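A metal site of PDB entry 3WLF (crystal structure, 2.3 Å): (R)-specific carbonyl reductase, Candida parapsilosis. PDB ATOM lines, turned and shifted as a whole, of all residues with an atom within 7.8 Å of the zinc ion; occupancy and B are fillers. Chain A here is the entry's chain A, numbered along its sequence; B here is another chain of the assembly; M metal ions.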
ATOM      1  N   ASN A  98      22.619  32.235   1.920  1.00  0.00           N
ATOM      2  CA  ASN A  98      22.704  32.352   3.381  1.00  0.00           C
ATOM      3  C   ASN A  98      21.725  31.423   4.115  1.00  0.00           C
ATOM      4  O   ASN A  98      20.924  31.874   4.922  1.00  0.00           O
ATOM      5  CB  ASN A  98      22.441  33.819   3.765  1.00  0.00           C
ATOM      6  CG  ASN A  98      22.721  34.102   5.226  1.00  0.00           C
ATOM      7  OD1 ASN A  98      23.762  33.713   5.766  1.00  0.00           O
ATOM      8  ND2 ASN A  98      21.811  34.810   5.879  1.00  0.00           N
ATOM      9  N   GLY A  99      21.822  30.123   3.828  1.00  0.00           N
ATOM     10  CA  GLY A  99      20.941  29.158   4.453  1.00  0.00           C
ATOM     11  C   GLY A  99      20.942  29.139   5.978  1.00  0.00           C
ATOM     12  O   GLY A  99      21.942  29.475   6.616  1.00  0.00           O
ATOM     13  N   CYS A 100      19.817  28.733   6.557  1.00  0.00           N
ATOM     14  CA  CYS A 100      19.677  28.670   8.012  1.00  0.00           C
ATOM     15  C   CYS A 100      20.670  27.685   8.616  1.00  0.00           C
ATOM     16  O   CYS A 100      21.112  27.848   9.754  1.00  0.00           O
ATOM     17  CB  CYS A 100      18.251  28.270   8.405  1.00  0.00           C
ATOM     18  SG  CYS A 100      17.878  26.500   8.274  1.00  0.00           S
ATOM     19  N   GLY A 101      20.990  26.641   7.854  1.00  0.00           N
ATOM     20  CA  GLY A 101      21.933  25.633   8.325  1.00  0.00           C
ATOM     21  C   GLY A 101      21.337  24.620   9.295  1.00  0.00           C
ATOM     22  O   GLY A 101      22.063  23.802   9.846  1.00  0.00           O
ATOM     23  N   GLY A 102      20.016  24.656   9.470  1.00  0.00           N
ATOM     24  CA  GLY A 102      19.386  23.732  10.398  1.00  0.00           C
ATOM     25  C   GLY A 102      18.348  22.797   9.808  1.00  0.00           C
ATOM     26  O   GLY A 102      18.150  21.687  10.323  1.00  0.00           O
ATOM     27  N   CYS A 103      17.673  23.216   8.741  1.00  0.00           N
ATOM     28  CA  CYS A 103      16.649  22.397   8.114  1.00  0.00           C
ATOM     29  C   CYS A 103      17.248  21.197   7.387  1.00  0.00           C
ATOM     30  O   CYS A 103      18.466  21.033   7.324  1.00  0.00           O
ATOM     31  CB  CYS A 103      15.841  23.229   7.122  1.00  0.00           C
ATOM     32  SG  CYS A 103      16.815  23.832   5.754  1.00  0.00           S
ATOM     33  N   LYS A 104      16.383  20.349   6.832  1.00  0.00           N
ATOM     34  CA  LYS A 104      16.844  19.166   6.113  1.00  0.00           C
ATOM     35  C   LYS A 104      17.547  19.524   4.817  1.00  0.00           C
ATOM     36  O   LYS A 104      18.441  18.811   4.366  1.00  0.00           O
ATOM     37  CB  LYS A 104      15.672  18.225   5.828  1.00  0.00           C
ATOM     38  CG  LYS A 104      14.627  18.784   4.876  1.00  0.00           C
ATOM     39  CD  LYS A 104      13.537  17.754   4.604  1.00  0.00           C
ATOM     40  CE  LYS A 104      12.467  18.288   3.664  1.00  0.00           C
ATOM     41  NZ  LYS A 104      11.406  17.271   3.399  1.00  0.00           N
ATOM     42  N   TYR A 105      17.147  20.644   4.210  1.00  0.00           N
ATOM     43  CA  TYR A 105      17.745  21.109   2.968  1.00  0.00           C
ATOM     44  C   TYR A 105      19.195  21.477   3.265  1.00  0.00           C
ATOM     45  O   TYR A 105      20.105  20.971   2.624  1.00  0.00           O
ATOM     46  CB  TYR A 105      16.947  22.282   2.410  1.00  0.00           C
ATOM     47  CG  TYR A 105      15.525  21.888   2.088  1.00  0.00           C
ATOM     48  CD1 TYR A 105      15.269  20.984   1.051  1.00  0.00           C
ATOM     49  CD2 TYR A 105      14.459  22.335   2.851  1.00  0.00           C
ATOM     50  CE1 TYR A 105      13.975  20.534   0.797  1.00  0.00           C
ATOM     51  CE2 TYR A 105      13.154  21.894   2.600  1.00  0.00           C
ATOM     52  CZ  TYR A 105      12.927  20.989   1.572  1.00  0.00           C
ATOM     53  OH  TYR A 105      11.650  20.533   1.331  1.00  0.00           O
ATOM     54  N   CYS A 106      19.399  22.360   4.230  1.00  0.00           N
ATOM     55  CA  CYS A 106      20.759  22.704   4.628  1.00  0.00           C
ATOM     56  C   CYS A 106      21.130  21.397   5.311  1.00  0.00           C
ATOM     57  O   CYS A 106      20.249  20.601   5.615  1.00  0.00           O
ATOM     58  CB  CYS A 106      20.774  23.830   5.659  1.00  0.00           C
ATOM     59  SG  CYS A 106      20.164  25.432   5.084  1.00  0.00           S
ATOM     60  N   ARG A 107      22.411  21.144   5.550  1.00  0.00           N
ATOM     61  CA  ARG A 107      22.774  19.892   6.217  1.00  0.00           C
ATOM     62  C   ARG A 107      22.546  18.719   5.264  1.00  0.00           C
ATOM     63  O   ARG A 107      23.079  17.626   5.461  1.00  0.00           O
ATOM     64  CB  ARG A 107      21.927  19.739   7.481  1.00  0.00           C
ATOM     65  CG  ARG A 107      21.700  18.304   7.910  1.00  0.00           C
ATOM     66  CD  ARG A 107      20.294  18.128   8.478  1.00  0.00           C
ATOM     67  NE  ARG A 107      20.068  18.875   9.704  1.00  0.00           N
ATOM     68  CZ  ARG A 107      18.976  18.770  10.451  1.00  0.00           C
ATOM     69  NH1 ARG A 107      17.993  17.956  10.080  1.00  0.00           N
ATOM     70  NH2 ARG A 107      18.843  19.479  11.552  1.00  0.00           N
ATOM     71  N   ILE A 110      22.269  20.912   0.335  1.00  0.00           N
ATOM     72  CA  ILE A 110      21.596  21.826  -0.572  1.00  0.00           C
ATOM     73  C   ILE A 110      21.057  23.058   0.156  1.00  0.00           C
ATOM     74  O   ILE A 110      19.866  23.345   0.140  1.00  0.00           O
ATOM     75  CB  ILE A 110      20.438  21.124  -1.333  1.00  0.00           C
ATOM     76  CG1 ILE A 110      19.438  20.532  -0.350  1.00  0.00           C
ATOM     77  CG2 ILE A 110      21.001  20.045  -2.235  1.00  0.00           C
ATOM     78  CD1 ILE A 110      18.261  19.845  -1.014  1.00  0.00           C
ATOM     79  N   ASP A 111      21.966  23.793   0.789  1.00  0.00           N
ATOM     80  CA  ASP A 111      21.598  24.995   1.536  1.00  0.00           C
ATOM     81  C   ASP A 111      21.166  26.146   0.635  1.00  0.00           C
ATOM     82  O   ASP A 111      20.789  27.206   1.126  1.00  0.00           O
ATOM     83  CB  ASP A 111      22.757  25.458   2.430  1.00  0.00           C
ATOM     84  CG  ASP A 111      24.071  25.585   1.679  1.00  0.00           C
ATOM     85  OD1 ASP A 111      24.047  25.909   0.481  1.00  0.00           O
ATOM     86  OD2 ASP A 111      25.126  25.357   2.299  1.00  0.00           O
ATOM     87  N   ASN A 112      21.223  25.941  -0.679  1.00  0.00           N
ATOM     88  CA  ASN A 112      20.837  26.999  -1.615  1.00  0.00           C
ATOM     89  C   ASN A 112      19.325  27.085  -1.817  1.00  0.00           C
ATOM     90  O   ASN A 112      18.823  28.082  -2.325  1.00  0.00           O
ATOM     91  CB  ASN A 112      21.538  26.800  -2.959  1.00  0.00           C
ATOM     92  CG  ASN A 112      21.147  25.510  -3.646  1.00  0.00           C
ATOM     93  OD1 ASN A 112      21.227  24.436  -3.058  1.00  0.00           O
ATOM     94  ND2 ASN A 112      20.735  25.608  -4.899  1.00  0.00           N
ATOM     95  N   VAL A 113      18.601  26.043  -1.414  1.00  0.00           N
ATOM     96  CA  VAL A 113      17.141  26.043  -1.549  1.00  0.00           C
ATOM     97  C   VAL A 113      16.472  26.008  -0.175  1.00  0.00           C
ATOM     98  O   VAL A 113      15.373  25.476  -0.019  1.00  0.00           O
ATOM     99  CB  VAL A 113      16.642  24.839  -2.382  1.00  0.00           C
ATOM    100  CG1 VAL A 113      17.215  24.898  -3.780  1.00  0.00           C
ATOM    101  CG2 VAL A 113      17.030  23.531  -1.698  1.00  0.00           C
ATOM    102  N   CYS A 114      17.144  26.580   0.816  1.00  0.00           N
ATOM    103  CA  CYS A 114      16.630  26.626   2.176  1.00  0.00           C
ATOM    104  C   CYS A 114      15.372  27.485   2.279  1.00  0.00           C
ATOM    105  O   CYS A 114      15.391  28.663   1.921  1.00  0.00           O
ATOM    106  CB  CYS A 114      17.707  27.180   3.117  1.00  0.00           C
ATOM    107  SG  CYS A 114      17.111  27.505   4.791  1.00  0.00           S
ATOM    108  N   LYS A 115      14.290  26.891   2.762  1.00  0.00           N
ATOM    109  CA  LYS A 115      13.028  27.612   2.902  1.00  0.00           C
ATOM    110  C   LYS A 115      13.069  28.699   3.972  1.00  0.00           C
ATOM    111  O   LYS A 115      12.471  29.770   3.794  1.00  0.00           O
ATOM    112  CB  LYS A 115      11.888  26.641   3.223  1.00  0.00           C
ATOM    113  CG  LYS A 115      11.473  25.758   2.066  1.00  0.00           C
ATOM    114  CD  LYS A 115      10.258  24.904   2.423  1.00  0.00           C
ATOM    115  CE  LYS A 115       9.812  24.061   1.234  1.00  0.00           C
ATOM    116  NZ  LYS A 115       8.601  23.265   1.546  1.00  0.00           N
ATOM    117  N   ASN A 116      13.764  28.440   5.074  1.00  0.00           N
ATOM    118  CA  ASN A 116      13.851  29.427   6.159  1.00  0.00           C
ATOM    119  C   ASN A 116      14.683  30.644   5.777  1.00  0.00           C
ATOM    120  O   ASN A 116      14.392  31.763   6.219  1.00  0.00           O
ATOM    121  CB  ASN A 116      14.450  28.781   7.414  1.00  0.00           C
ATOM    122  CG  ASN A 116      13.636  27.616   7.925  1.00  0.00           C
ATOM    123  OD1 ASN A 116      12.400  27.678   7.969  1.00  0.00           O
ATOM    124  ND2 ASN A 116      14.310  26.545   8.335  1.00  0.00           N
ATOM    125  N   ALA A 117      15.707  30.436   4.963  1.00  0.00           N
ATOM    126  CA  ALA A 117      16.579  31.530   4.533  1.00  0.00           C
ATOM    127  C   ALA A 117      15.914  32.417   3.486  1.00  0.00           C
ATOM    128  O   ALA A 117      16.458  33.443   3.091  1.00  0.00           O
ATOM    129  CB  ALA A 117      17.894  30.970   3.988  1.00  0.00           C
ATOM    130  N   PHE A 118      14.725  32.014   3.049  1.00  0.00           N
ATOM    131  CA  PHE A 118      13.994  32.783   2.051  1.00  0.00           C
ATOM    132  C   PHE A 118      13.718  34.179   2.590  1.00  0.00           C
ATOM    133  O   PHE A 118      13.137  34.340   3.664  1.00  0.00           O
ATOM    134  CB  PHE A 118      12.682  32.085   1.704  1.00  0.00           C
ATOM    135  CG  PHE A 118      12.346  32.113   0.244  1.00  0.00           C
ATOM    136  CD1 PHE A 118      12.148  33.319  -0.418  1.00  0.00           C
ATOM    137  CD2 PHE A 118      12.258  30.934  -0.492  1.00  0.00           C
ATOM    138  CE1 PHE A 118      11.862  33.358  -1.781  1.00  0.00           C
ATOM    139  CE2 PHE A 118      11.976  30.951  -1.847  1.00  0.00           C
ATOM    140  CZ  PHE A 118      11.779  32.166  -2.498  1.00  0.00           C
ATOM    141  N   ARG A 138      25.544  34.077  10.407  1.00  0.00           N
ATOM    142  CA  ARG A 138      25.838  32.650  10.314  1.00  0.00           C
ATOM    143  C   ARG A 138      27.118  32.385   9.511  1.00  0.00           C
ATOM    144  O   ARG A 138      27.078  32.130   8.310  1.00  0.00           O
ATOM    145  CB  ARG A 138      24.657  31.916   9.669  1.00  0.00           C
ATOM    146  CG  ARG A 138      23.361  32.012  10.479  1.00  0.00           C
ATOM    147  CD  ARG A 138      22.287  31.066   9.952  1.00  0.00           C
ATOM    148  NE  ARG A 138      21.688  31.519   8.696  1.00  0.00           N
ATOM    149  CZ  ARG A 138      20.879  32.570   8.592  1.00  0.00           C
ATOM    150  NH1 ARG A 138      20.381  32.905   7.407  1.00  0.00           N
ATOM    151  NH2 ARG A 138      20.562  33.285   9.657  1.00  0.00           N
ATOM    152  N   ARG A 140      28.680  30.084   8.859  1.00  0.00           N
ATOM    153  CA  ARG A 140      28.597  28.868   8.071  1.00  0.00           C
ATOM    154  C   ARG A 140      28.583  29.163   6.573  1.00  0.00           C
ATOM    155  O   ARG A 140      29.147  28.413   5.772  1.00  0.00           O
ATOM    156  CB  ARG A 140      27.322  28.098   8.445  1.00  0.00           C
ATOM    157  CG  ARG A 140      26.953  26.977   7.491  1.00  0.00           C
ATOM    158  CD  ARG A 140      25.591  26.383   7.854  1.00  0.00           C
ATOM    159  NE  ARG A 140      25.232  25.272   6.981  1.00  0.00           N
ATOM    160  CZ  ARG A 140      24.903  25.396   5.697  1.00  0.00           C
ATOM    161  NH1 ARG A 140      24.601  24.319   4.985  1.00  0.00           N
ATOM    162  NH2 ARG A 140      24.871  26.599   5.133  1.00  0.00           N
ATOM    163  N   ASN B  85      13.691  28.550  14.766  1.00  0.00           N
ATOM    164  CA  ASN B  85      13.317  27.230  14.274  1.00  0.00           C
ATOM    165  C   ASN B  85      12.683  26.405  15.394  1.00  0.00           C
ATOM    166  O   ASN B  85      11.801  25.579  15.137  1.00  0.00           O
ATOM    167  CB  ASN B  85      14.540  26.483  13.733  1.00  0.00           C
ATOM    168  CG  ASN B  85      15.253  27.262  12.629  1.00  0.00           C
ATOM    169  OD1 ASN B  85      14.625  27.748  11.697  1.00  0.00           O
ATOM    170  ND2 ASN B  85      16.575  27.361  12.744  1.00  0.00           N
HETATM  171 ZN    ZN M   1      18.070  25.686   6.005  1.00  0.00          ZN
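Merely in contact with the zinc ion: Gly 101 (3.6 Å). The nearest printed residue that does not touch the zinc ion is Gly 102 (4.1 Å).
The zinc ion is bound by the side-chain sulfur of Cys 103 (2.3 Å), the side-chain sulfur of Cys 106 (2.3 Å), the side-chain sulfur of Cys 114 (2.4 Å) and the side-chain sulfur of Cys 100 (2.4 Å). The zinc ion has four donor atoms within binding distance.
N of Tyr 105 lies close to SG of Cys 103 (3.6 Å). The side-chain sulfur (SG) of Cys 106 lies close to the backbone NH (N) of Gly 101 (3.1 Å). SG of Cys 114 lies close to N of Asn 116 (3.5 Å). The side-chain sulfur (SG) of Cys 114 sits close to the backbone NH (N) of Ala 117 (3.3 Å). SG of Cys 100 lies close to N of Gly 102, 3.1 Å away. The side-chain sulfur (SG) of Cys 100 sits close to the side-chain amide nitrogen (ND2) of Asn 116, 3.6 Å away.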
